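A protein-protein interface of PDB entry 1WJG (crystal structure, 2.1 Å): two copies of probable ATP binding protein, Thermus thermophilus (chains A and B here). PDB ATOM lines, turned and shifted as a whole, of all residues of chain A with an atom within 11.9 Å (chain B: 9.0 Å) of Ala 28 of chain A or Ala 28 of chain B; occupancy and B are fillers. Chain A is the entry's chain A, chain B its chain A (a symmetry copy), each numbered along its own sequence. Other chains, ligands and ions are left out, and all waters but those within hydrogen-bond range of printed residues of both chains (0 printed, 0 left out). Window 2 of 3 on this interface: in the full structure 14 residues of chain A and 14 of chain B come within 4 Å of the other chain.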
ATOM      1  N   PHE A   2       9.880 -31.044   5.326  1.00  0.00           N
ATOM      2  CA  PHE A   2       8.449 -30.897   5.737  1.00  0.00           C
ATOM      3  C   PHE A   2       7.511 -31.602   4.756  1.00  0.00           C
ATOM      4  O   PHE A   2       7.378 -31.182   3.605  1.00  0.00           O
ATOM      5  CB  PHE A   2       8.062 -29.410   5.829  1.00  0.00           C
ATOM      6  CG  PHE A   2       8.825 -28.634   6.881  1.00  0.00           C
ATOM      7  CD1 PHE A   2       9.131 -27.292   6.680  1.00  0.00           C
ATOM      8  CD2 PHE A   2       9.215 -29.236   8.073  1.00  0.00           C
ATOM      9  CE1 PHE A   2       9.815 -26.556   7.655  1.00  0.00           C
ATOM     10  CE2 PHE A   2       9.900 -28.509   9.058  1.00  0.00           C
ATOM     11  CZ  PHE A   2      10.199 -27.168   8.848  1.00  0.00           C
ATOM     12  N   LYS A   3       6.849 -32.660   5.225  1.00  0.00           N
ATOM     13  CA  LYS A   3       5.913 -33.434   4.403  1.00  0.00           C
ATOM     14  C   LYS A   3       4.449 -33.094   4.678  1.00  0.00           C
ATOM     15  O   LYS A   3       3.592 -33.261   3.812  1.00  0.00           O
ATOM     16  CB  LYS A   3       6.115 -34.938   4.608  1.00  0.00           C
ATOM     17  CG  LYS A   3       7.299 -35.538   3.871  1.00  0.00           C
ATOM     18  CD  LYS A   3       8.620 -35.245   4.568  1.00  0.00           C
ATOM     19  CE  LYS A   3       9.767 -35.982   3.890  1.00  0.00           C
ATOM     20  NZ  LYS A   3       9.489 -37.444   3.783  1.00  0.00           N
ATOM     21  N   THR A   4       4.160 -32.683   5.908  1.00  0.00           N
ATOM     22  CA  THR A   4       2.804 -32.315   6.303  1.00  0.00           C
ATOM     23  C   THR A   4       2.883 -31.044   7.151  1.00  0.00           C
ATOM     24  O   THR A   4       3.599 -31.000   8.158  1.00  0.00           O
ATOM     25  CB  THR A   4       2.100 -33.450   7.103  1.00  0.00           C
ATOM     26  OG1 THR A   4       2.849 -33.748   8.280  1.00  0.00           O
ATOM     27  CG2 THR A   4       1.987 -34.720   6.269  1.00  0.00           C
ATOM     28  N   ILE A   5       2.203 -29.995   6.701  1.00  0.00           N
ATOM     29  CA  ILE A   5       2.201 -28.717   7.403  1.00  0.00           C
ATOM     30  C   ILE A   5       0.820 -28.431   7.971  1.00  0.00           C
ATOM     31  O   ILE A   5      -0.176 -28.547   7.266  1.00  0.00           O
ATOM     32  CB  ILE A   5       2.603 -27.570   6.454  1.00  0.00           C
ATOM     33  CG1 ILE A   5       4.033 -27.791   5.952  1.00  0.00           C
ATOM     34  CG2 ILE A   5       2.463 -26.220   7.159  1.00  0.00           C
ATOM     35  CD1 ILE A   5       4.431 -26.868   4.844  1.00  0.00           C
ATOM     36  N   ALA A  19      -2.083 -17.929   7.000  1.00  0.00           N
ATOM     37  CA  ALA A  19      -2.626 -18.799   5.957  1.00  0.00           C
ATOM     38  C   ALA A  19      -1.849 -18.628   4.661  1.00  0.00           C
ATOM     39  O   ALA A  19      -1.492 -19.606   4.013  1.00  0.00           O
ATOM     40  CB  ALA A  19      -4.094 -18.502   5.735  1.00  0.00           C
ATOM     41  N   GLU A  20      -1.574 -17.376   4.308  1.00  0.00           N
ATOM     42  CA  GLU A  20      -0.824 -17.047   3.103  1.00  0.00           C
ATOM     43  C   GLU A  20       0.577 -17.661   3.199  1.00  0.00           C
ATOM     44  O   GLU A  20       1.071 -18.250   2.235  1.00  0.00           O
ATOM     45  CB  GLU A  20      -0.741 -15.523   2.939  1.00  0.00           C
ATOM     46  CG  GLU A  20      -0.135 -15.060   1.609  1.00  0.00           C
ATOM     47  CD  GLU A  20      -0.055 -13.537   1.470  1.00  0.00           C
ATOM     48  OE1 GLU A  20       0.498 -13.065   0.448  1.00  0.00           O
ATOM     49  OE2 GLU A  20      -0.541 -12.811   2.372  1.00  0.00           O
ATOM     50  N   VAL A  21       1.192 -17.567   4.379  1.00  0.00           N
ATOM     51  CA  VAL A  21       2.526 -18.131   4.589  1.00  0.00           C
ATOM     52  C   VAL A  21       2.492 -19.655   4.463  1.00  0.00           C
ATOM     53  O   VAL A  21       3.325 -20.245   3.778  1.00  0.00           O
ATOM     54  CB  VAL A  21       3.118 -17.734   5.971  1.00  0.00           C
ATOM     55  CG1 VAL A  21       4.416 -18.497   6.231  1.00  0.00           C
ATOM     56  CG2 VAL A  21       3.389 -16.232   6.017  1.00  0.00           C
ATOM     57  N   ALA A  22       1.518 -20.280   5.118  1.00  0.00           N
ATOM     58  CA  ALA A  22       1.351 -21.733   5.088  1.00  0.00           C
ATOM     59  C   ALA A  22       1.162 -22.275   3.670  1.00  0.00           C
ATOM     60  O   ALA A  22       1.729 -23.308   3.311  1.00  0.00           O
ATOM     61  CB  ALA A  22       0.157 -22.140   5.958  1.00  0.00           C
ATOM     62  N   LYS A  23       0.343 -21.591   2.879  1.00  0.00           N
ATOM     63  CA  LYS A  23       0.079 -22.022   1.507  1.00  0.00           C
ATOM     64  C   LYS A  23       1.363 -22.021   0.682  1.00  0.00           C
ATOM     65  O   LYS A  23       1.653 -22.980  -0.038  1.00  0.00           O
ATOM     66  CB  LYS A  23      -0.978 -21.120   0.867  1.00  0.00           C
ATOM     67  CG  LYS A  23      -1.373 -21.522  -0.544  1.00  0.00           C
ATOM     68  CD  LYS A  23      -2.435 -20.588  -1.100  1.00  0.00           C
ATOM     69  CE  LYS A  23      -2.852 -21.006  -2.499  1.00  0.00           C
ATOM     70  NZ  LYS A  23      -4.027 -20.225  -2.990  1.00  0.00           N
ATOM     71  N   ALA A  24       2.146 -20.955   0.835  1.00  0.00           N
ATOM     72  CA  ALA A  24       3.415 -20.800   0.137  1.00  0.00           C
ATOM     73  C   ALA A  24       4.393 -21.868   0.613  1.00  0.00           C
ATOM     74  O   ALA A  24       5.107 -22.467  -0.183  1.00  0.00           O
ATOM     75  CB  ALA A  24       3.987 -19.410   0.398  1.00  0.00           C
ATOM     76  N   GLU A  25       4.383 -22.125   1.917  1.00  0.00           N
ATOM     77  CA  GLU A  25       5.254 -23.120   2.530  1.00  0.00           C
ATOM     78  C   GLU A  25       4.985 -24.533   1.986  1.00  0.00           C
ATOM     79  O   GLU A  25       5.917 -25.271   1.655  1.00  0.00           O
ATOM     80  CB  GLU A  25       5.054 -23.085   4.048  1.00  0.00           C
ATOM     81  CG  GLU A  25       6.098 -23.818   4.855  1.00  0.00           C
ATOM     82  CD  GLU A  25       7.464 -23.149   4.838  1.00  0.00           C
ATOM     83  OE1 GLU A  25       8.414 -23.786   5.330  1.00  0.00           O
ATOM     84  OE2 GLU A  25       7.596 -22.005   4.344  1.00  0.00           O
ATOM     85  N   ALA A  26       3.711 -24.906   1.898  1.00  0.00           N
ATOM     86  CA  ALA A  26       3.332 -26.226   1.394  1.00  0.00           C
ATOM     87  C   ALA A  26       3.723 -26.371  -0.071  1.00  0.00           C
ATOM     88  O   ALA A  26       4.217 -27.417  -0.491  1.00  0.00           O
ATOM     89  CB  ALA A  26       1.827 -26.453   1.569  1.00  0.00           C
ATOM     90  N   GLU A  27       3.507 -25.309  -0.841  1.00  0.00           N
ATOM     91  CA  GLU A  27       3.839 -25.299  -2.264  1.00  0.00           C
ATOM     92  C   GLU A  27       5.357 -25.432  -2.453  1.00  0.00           C
ATOM     93  O   GLU A  27       5.817 -26.171  -3.322  1.00  0.00           O
ATOM     94  CB  GLU A  27       3.319 -24.003  -2.905  1.00  0.00           C
ATOM     95  CG  GLU A  27       3.260 -23.990  -4.434  1.00  0.00           C
ATOM     96  CD  GLU A  27       4.621 -23.845  -5.102  1.00  0.00           C
ATOM     97  OE1 GLU A  27       5.511 -23.173  -4.534  1.00  0.00           O
ATOM     98  OE2 GLU A  27       4.802 -24.402  -6.206  1.00  0.00           O
ATOM     99  N   ALA A  28       6.126 -24.753  -1.602  1.00  0.00           N
ATOM    100  CA  ALA A  28       7.586 -24.792  -1.678  1.00  0.00           C
ATOM    101  C   ALA A  28       8.178 -26.146  -1.301  1.00  0.00           C
ATOM    102  O   ALA A  28       9.174 -26.583  -1.889  1.00  0.00           O
ATOM    103  CB  ALA A  28       8.193 -23.689  -0.801  1.00  0.00           C
ATOM    104  N   HIS A  29       7.572 -26.813  -0.326  1.00  0.00           N
ATOM    105  CA  HIS A  29       8.059 -28.113   0.122  1.00  0.00           C
ATOM    106  C   HIS A  29       7.350 -29.296  -0.534  1.00  0.00           C
ATOM    107  O   HIS A  29       7.770 -30.442  -0.354  1.00  0.00           O
ATOM    108  CB  HIS A  29       7.912 -28.239   1.641  1.00  0.00           C
ATOM    109  CG  HIS A  29       8.826 -27.343   2.417  1.00  0.00           C
ATOM    110  ND1 HIS A  29      10.054 -27.759   2.880  1.00  0.00           N
ATOM    111  CD2 HIS A  29       8.682 -26.061   2.826  1.00  0.00           C
ATOM    112  CE1 HIS A  29      10.628 -26.771   3.545  1.00  0.00           C
ATOM    113  NE2 HIS A  29       9.816 -25.729   3.527  1.00  0.00           N
ATOM    114  N   GLY A  30       6.287 -29.017  -1.286  1.00  0.00           N
ATOM    115  CA  GLY A  30       5.514 -30.080  -1.913  1.00  0.00           C
ATOM    116  C   GLY A  30       4.827 -30.903  -0.834  1.00  0.00           C
ATOM    117  O   GLY A  30       4.633 -32.112  -0.980  1.00  0.00           O
ATOM    118  N   ALA A  31       4.453 -30.238   0.257  1.00  0.00           N
ATOM    119  CA  ALA A  31       3.816 -30.900   1.391  1.00  0.00           C
ATOM    120  C   ALA A  31       2.294 -30.814   1.425  1.00  0.00           C
ATOM    121  O   ALA A  31       1.688 -29.987   0.745  1.00  0.00           O
ATOM    122  CB  ALA A  31       4.386 -30.345   2.690  1.00  0.00           C
ATOM    123  N   ARG A  32       1.677 -31.716   2.184  1.00  0.00           N
ATOM    124  CA  ARG A  32       0.227 -31.694   2.342  1.00  0.00           C
ATOM    125  C   ARG A  32      -0.070 -30.650   3.419  1.00  0.00           C
ATOM    126  O   ARG A  32       0.592 -30.623   4.461  1.00  0.00           O
ATOM    127  CB  ARG A  32      -0.315 -33.056   2.780  1.00  0.00           C
ATOM    128  CG  ARG A  32      -1.841 -33.050   2.938  1.00  0.00           C
ATOM    129  CD  ARG A  32      -2.426 -34.440   3.090  1.00  0.00           C
ATOM    130  NE  ARG A  32      -2.058 -35.056   4.361  1.00  0.00           N
ATOM    131  CZ  ARG A  32      -2.872 -35.163   5.409  1.00  0.00           C
ATOM    132  NH1 ARG A  32      -2.442 -35.742   6.525  1.00  0.00           N
ATOM    133  NH2 ARG A  32      -4.110 -34.690   5.350  1.00  0.00           N
ATOM    134  N   LEU A  33      -1.029 -29.772   3.150  1.00  0.00           N
ATOM    135  CA  LEU A  33      -1.398 -28.717   4.096  1.00  0.00           C
ATOM    136  C   LEU A  33      -2.699 -29.054   4.810  1.00  0.00           C
ATOM    137  O   LEU A  33      -3.733 -29.260   4.169  1.00  0.00           O
ATOM    138  CB  LEU A  33      -1.588 -27.388   3.362  1.00  0.00           C
ATOM    139  CG  LEU A  33      -1.251 -26.049   4.041  1.00  0.00           C
ATOM    140  CD1 LEU A  33      -2.125 -24.960   3.440  1.00  0.00           C
ATOM    141  CD2 LEU A  33      -1.416 -26.103   5.551  1.00  0.00           C
ATOM    142  N   THR A  73      -6.609 -21.221   1.447  1.00  0.00           N
ATOM    143  CA  THR A  73      -5.543 -22.178   1.158  1.00  0.00           C
ATOM    144  C   THR A  73      -5.812 -23.165   0.025  1.00  0.00           C
ATOM    145  O   THR A  73      -4.871 -23.749  -0.521  1.00  0.00           O
ATOM    146  CB  THR A  73      -5.177 -22.992   2.423  1.00  0.00           C
ATOM    147  OG1 THR A  73      -6.329 -23.702   2.885  1.00  0.00           O
ATOM    148  CG2 THR A  73      -4.673 -22.070   3.535  1.00  0.00           C
ATOM    149  N   LEU A 102       5.502 -29.435  10.731  1.00  0.00           N
ATOM    150  CA  LEU A 102       5.600 -27.998  10.922  1.00  0.00           C
ATOM    151  C   LEU A 102       4.240 -27.415  11.246  1.00  0.00           C
ATOM    152  O   LEU A 102       3.241 -27.765  10.616  1.00  0.00           O
ATOM    153  CB  LEU A 102       6.109 -27.329   9.638  1.00  0.00           C
ATOM    154  CG  LEU A 102       6.097 -25.796   9.616  1.00  0.00           C
ATOM    155  CD1 LEU A 102       7.148 -25.260  10.576  1.00  0.00           C
ATOM    156  CD2 LEU A 102       6.353 -25.275   8.206  1.00  0.00           C
ATOM    157  N   VAL A 104       2.210 -23.809  11.501  1.00  0.00           N
ATOM    158  CA  VAL A 104       2.273 -22.407  11.092  1.00  0.00           C
ATOM    159  C   VAL A 104       1.120 -21.693  11.785  1.00  0.00           C
ATOM    160  O   VAL A 104      -0.017 -22.150  11.734  1.00  0.00           O
ATOM    161  CB  VAL A 104       2.142 -22.257   9.560  1.00  0.00           C
ATOM    162  CG1 VAL A 104       2.219 -20.795   9.157  1.00  0.00           C
ATOM    163  CG2 VAL A 104       3.242 -23.040   8.867  1.00  0.00           C
ATOM    164  N   LEU A 134       6.301 -22.070  12.999  1.00  0.00           N
ATOM    165  CA  LEU A 134       6.504 -20.873  12.196  1.00  0.00           C
ATOM    166  C   LEU A 134       5.523 -19.810  12.681  1.00  0.00           C
ATOM    167  O   LEU A 134       4.311 -19.905  12.461  1.00  0.00           O
ATOM    168  CB  LEU A 134       6.281 -21.175  10.714  1.00  0.00           C
ATOM    169  CG  LEU A 134       7.151 -20.369   9.743  1.00  0.00           C
ATOM    170  CD1 LEU A 134       6.879 -20.804   8.310  1.00  0.00           C
ATOM    171  CD2 LEU A 134       6.902 -18.897   9.904  1.00  0.00           C
ATOM    172  N   PHE B   2       9.580 -16.210   0.475  1.00  0.00           N
ATOM    173  CA  PHE B   2      10.882 -15.995   1.180  1.00  0.00           C
ATOM    174  C   PHE B   2      12.047 -15.929   0.191  1.00  0.00           C
ATOM    175  O   PHE B   2      12.388 -16.929  -0.444  1.00  0.00           O
ATOM    176  CB  PHE B   2      11.140 -17.122   2.195  1.00  0.00           C
ATOM    177  CG  PHE B   2      10.126 -17.192   3.316  1.00  0.00           C
ATOM    178  CD1 PHE B   2       9.779 -18.419   3.873  1.00  0.00           C
ATOM    179  CD2 PHE B   2       9.539 -16.038   3.825  1.00  0.00           C
ATOM    180  CE1 PHE B   2       8.860 -18.495   4.927  1.00  0.00           C
ATOM    181  CE2 PHE B   2       8.618 -16.102   4.881  1.00  0.00           C
ATOM    182  CZ  PHE B   2       8.280 -17.332   5.432  1.00  0.00           C
ATOM    183  N   ILE B   5      16.719 -15.748   3.754  1.00  0.00           N
ATOM    184  CA  ILE B   5      16.489 -16.377   5.049  1.00  0.00           C
ATOM    185  C   ILE B   5      17.700 -16.187   5.948  1.00  0.00           C
ATOM    186  O   ILE B   5      18.826 -16.435   5.531  1.00  0.00           O
ATOM    187  CB  ILE B   5      16.216 -17.885   4.884  1.00  0.00           C
ATOM    188  CG1 ILE B   5      14.939 -18.094   4.065  1.00  0.00           C
ATOM    189  CG2 ILE B   5      16.117 -18.562   6.252  1.00  0.00           C
ATOM    190  CD1 ILE B   5      14.718 -19.513   3.645  1.00  0.00           C
ATOM    191  N   VAL B  21      17.351 -27.112   9.348  1.00  0.00           N
ATOM    192  CA  VAL B  21      16.043 -26.623   8.910  1.00  0.00           C
ATOM    193  C   VAL B  21      16.204 -25.457   7.933  1.00  0.00           C
ATOM    194  O   VAL B  21      15.573 -25.432   6.879  1.00  0.00           O
ATOM    195  CB  VAL B  21      15.153 -26.182  10.107  1.00  0.00           C
ATOM    196  CG1 VAL B  21      13.883 -25.500   9.600  1.00  0.00           C
ATOM    197  CG2 VAL B  21      14.778 -27.393  10.959  1.00  0.00           C
ATOM    198  N   ALA B  22      17.062 -24.504   8.288  1.00  0.00           N
ATOM    199  CA  ALA B  22      17.329 -23.331   7.456  1.00  0.00           C
ATOM    200  C   ALA B  22      17.842 -23.701   6.063  1.00  0.00           C
ATOM    201  O   ALA B  22      17.433 -23.110   5.063  1.00  0.00           O
ATOM    202  CB  ALA B  22      18.342 -22.416   8.151  1.00  0.00           C
ATOM    203  N   LYS B  23      18.760 -24.661   6.006  1.00  0.00           N
ATOM    204  CA  LYS B  23      19.330 -25.090   4.730  1.00  0.00           C
ATOM    205  C   LYS B  23      18.248 -25.656   3.816  1.00  0.00           C
ATOM    206  O   LYS B  23      18.178 -25.315   2.632  1.00  0.00           O
ATOM    207  CB  LYS B  23      20.434 -26.122   4.968  1.00  0.00           C
ATOM    208  CG  LYS B  23      21.138 -26.589   3.706  1.00  0.00           C
ATOM    209  CD  LYS B  23      22.227 -27.598   4.029  1.00  0.00           C
ATOM    210  CE  LYS B  23      22.951 -28.043   2.771  1.00  0.00           C
ATOM    211  NZ  LYS B  23      24.148 -28.882   3.081  1.00  0.00           N
ATOM    212  N   ALA B  24      17.380 -26.485   4.393  1.00  0.00           N
ATOM    213  CA  ALA B  24      16.275 -27.101   3.670  1.00  0.00           C
ATOM    214  C   ALA B  24      15.294 -26.024   3.223  1.00  0.00           C
ATOM    215  O   ALA B  24      14.802 -26.047   2.101  1.00  0.00           O
ATOM    216  CB  ALA B  24      15.569 -28.116   4.565  1.00  0.00           C
ATOM    217  N   GLU B  25      15.052 -25.057   4.103  1.00  0.00           N
ATOM    218  CA  GLU B  25      14.141 -23.952   3.829  1.00  0.00           C
ATOM    219  C   GLU B  25      14.612 -23.104   2.635  1.00  0.00           C
ATOM    220  O   GLU B  25      13.819 -22.760   1.754  1.00  0.00           O
ATOM    221  CB  GLU B  25      14.020 -23.086   5.086  1.00  0.00           C
ATOM    222  CG  GLU B  25      12.884 -22.093   5.079  1.00  0.00           C
ATOM    223  CD  GLU B  25      11.509 -22.737   5.172  1.00  0.00           C
ATOM    224  OE1 GLU B  25      10.522 -21.999   4.993  1.00  0.00           O
ATOM    225  OE2 GLU B  25      11.405 -23.962   5.420  1.00  0.00           O
ATOM    226  N   ALA B  26      15.898 -22.767   2.613  1.00  0.00           N
ATOM    227  CA  ALA B  26      16.460 -21.962   1.528  1.00  0.00           C
ATOM    228  C   ALA B  26      16.391 -22.721   0.209  1.00  0.00           C
ATOM    229  O   ALA B  26      16.067 -22.150  -0.831  1.00  0.00           O
ATOM    230  CB  ALA B  26      17.908 -21.575   1.846  1.00  0.00           C
ATOM    231  N   GLU B  27      16.690 -24.015   0.264  1.00  0.00           N
ATOM    232  CA  GLU B  27      16.660 -24.872  -0.920  1.00  0.00           C
ATOM    233  C   GLU B  27      15.226 -24.975  -1.459  1.00  0.00           C
ATOM    234  O   GLU B  27      15.007 -24.911  -2.668  1.00  0.00           O
ATOM    235  CB  GLU B  27      17.213 -26.261  -0.565  1.00  0.00           C
ATOM    236  CG  GLU B  27      17.586 -27.155  -1.749  1.00  0.00           C
ATOM    237  CD  GLU B  27      16.386 -27.751  -2.473  1.00  0.00           C
ATOM    238  OE1 GLU B  27      15.355 -28.027  -1.818  1.00  0.00           O
ATOM    239  OE2 GLU B  27      16.475 -27.953  -3.703  1.00  0.00           O
ATOM    240  N   ALA B  28      14.254 -25.084  -0.554  1.00  0.00           N
ATOM    241  CA  ALA B  28      12.848 -25.194  -0.939  1.00  0.00           C
ATOM    242  C   ALA B  28      12.282 -23.917  -1.550  1.00  0.00           C
ATOM    243  O   ALA B  28      11.461 -23.971  -2.472  1.00  0.00           O
ATOM    244  CB  ALA B  28      12.000 -25.621   0.267  1.00  0.00           C
ATOM    245  N   HIS B  29      12.718 -22.769  -1.044  1.00  0.00           N
ATOM    246  CA  HIS B  29      12.237 -21.486  -1.546  1.00  0.00           C
ATOM    247  C   HIS B  29      13.143 -20.860  -2.603  1.00  0.00           C
ATOM    248  O   HIS B  29      12.773 -19.853  -3.213  1.00  0.00           O
ATOM    249  CB  HIS B  29      12.075 -20.493  -0.393  1.00  0.00           C
ATOM    250  CG  HIS B  29      10.962 -20.831   0.549  1.00  0.00           C
ATOM    251  ND1 HIS B  29       9.695 -20.307   0.419  1.00  0.00           N
ATOM    252  CD2 HIS B  29      10.931 -21.624   1.645  1.00  0.00           C
ATOM    253  CE1 HIS B  29       8.932 -20.761   1.397  1.00  0.00           C
ATOM    254  NE2 HIS B  29       9.657 -21.563   2.156  1.00  0.00           N
ATOM    255  N   GLY B  30      14.318 -21.451  -2.814  1.00  0.00           N
ATOM    256  CA  GLY B  30      15.273 -20.901  -3.764  1.00  0.00           C
ATOM    257  C   GLY B  30      15.776 -19.560  -3.251  1.00  0.00           C
ATOM    258  O   GLY B  30      16.077 -18.651  -4.027  1.00  0.00           O
ATOM    259  N   ALA B  31      15.871 -19.441  -1.928  1.00  0.00           N
ATOM    260  CA  ALA B  31      16.303 -18.203  -1.287  1.00  0.00           C
ATOM    261  C   ALA B  31      17.776 -18.151  -0.896  1.00  0.00           C
ATOM    262  O   ALA B  31      18.452 -19.176  -0.826  1.00  0.00           O
ATOM    263  CB  ALA B  31      15.440 -17.938  -0.060  1.00  0.00           C
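The side-chain carboxylate (OE2) of Glu 25 of chain A sits at hydrogen-bond distance from a ring nitrogen (NE2) of His 29 of chain B (3.0 Å).
A ring nitrogen (NE2) of His 29 of chain A is in hydrogen-bond range of the side-chain carboxylate (OE2) of Glu 25 of chain B, 3.0 Å away.
OE1 of Glu 25 of chain A lies close to OE1 of Glu 25 of chain B, 2.8 Å away.
The side-chain carboxylate of Glu 25 of chain A is in hydrogen-bond range of a ring nitrogen (NE2) of His 29 of chain A.
OE1 of Glu 25 of chain B lies within hydrogen-bond range of NE2 of His 29 of chain B (3.0 Å).
Among the printed residues, pairs that only touch across the chains: Ala 28 of chain A with Ala 28 of chain B, His 29 of chain A with Ala 28 of chain B, Ala 28 of chain A with His 29 of chain B, Phe 2 of chain A with Glu 25 of chain B and Glu 25 of chain A with Phe 2 of chain B.
Of the printed residues of chain B, Ala 28 of chain A touches Ala 28 (3.5 Å) and His 29 (3.7 Å).
No residue of chain B comes within 4 Å of Glu 27 of chain A.
Of the printed residues of chain B, His 29 of chain A touches Glu 25 (3.0 Å) and Ala 28 (3.7 Å).
No residue of chain A comes within 4 Å of Ala 24 of chain B.
Glu 25 of chain B touches three residues of chain A.
Glu 27 of chain B touches none of the printed residues of chain A.
Gly 30 of chain B touches none of the printed residues of chain A.
No residue of chain A comes within 4 Å of Ala 31 of chain B.
Of the printed residues of chain A, Phe 2 of chain B touches Glu 25.
Of the printed residues of chain B, Glu 25 of chain A touches Phe 2, Glu 25 and His 29.
Of the printed residues of chain B, Phe 2 of chain A touches Glu 25 (3.8 Å).
The nearest printed residue of chain B that does not touch Phe 2 of chain A is Val 21 of chain B (4.1 Å).
Of the 23 printed residues of chain A, 4 touch a printed residue of chain B.
Hydrophobic or aromatic side chains of chain A within 4 Å of the printed part of chain B: Phe 2, Ala 28 and His 29.
Hydrophobic or aromatic side chains of chain B that line the printed part of chain A: Phe 2, Ala 28 and His 29.
Among the printed residues, no Asp or Glu carboxylate lies within 4 Å of a Lys or Arg side-chain nitrogen of the other chain.
Phe 2 of chain A touches Glu 25 of chain B, and with the chains exchanged Glu 25 of chain A touches Phe 2 of chain B.
Glu 25 of chain A touches its own counterpart, Glu 25 of chain B.
Ala 28 of chain A touches its own counterpart, Ala 28 of chain B.
Ala 28 of chain A touches His 29 of chain B, and with the chains exchanged His 29 of chain A touches Ala 28 of chain B.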
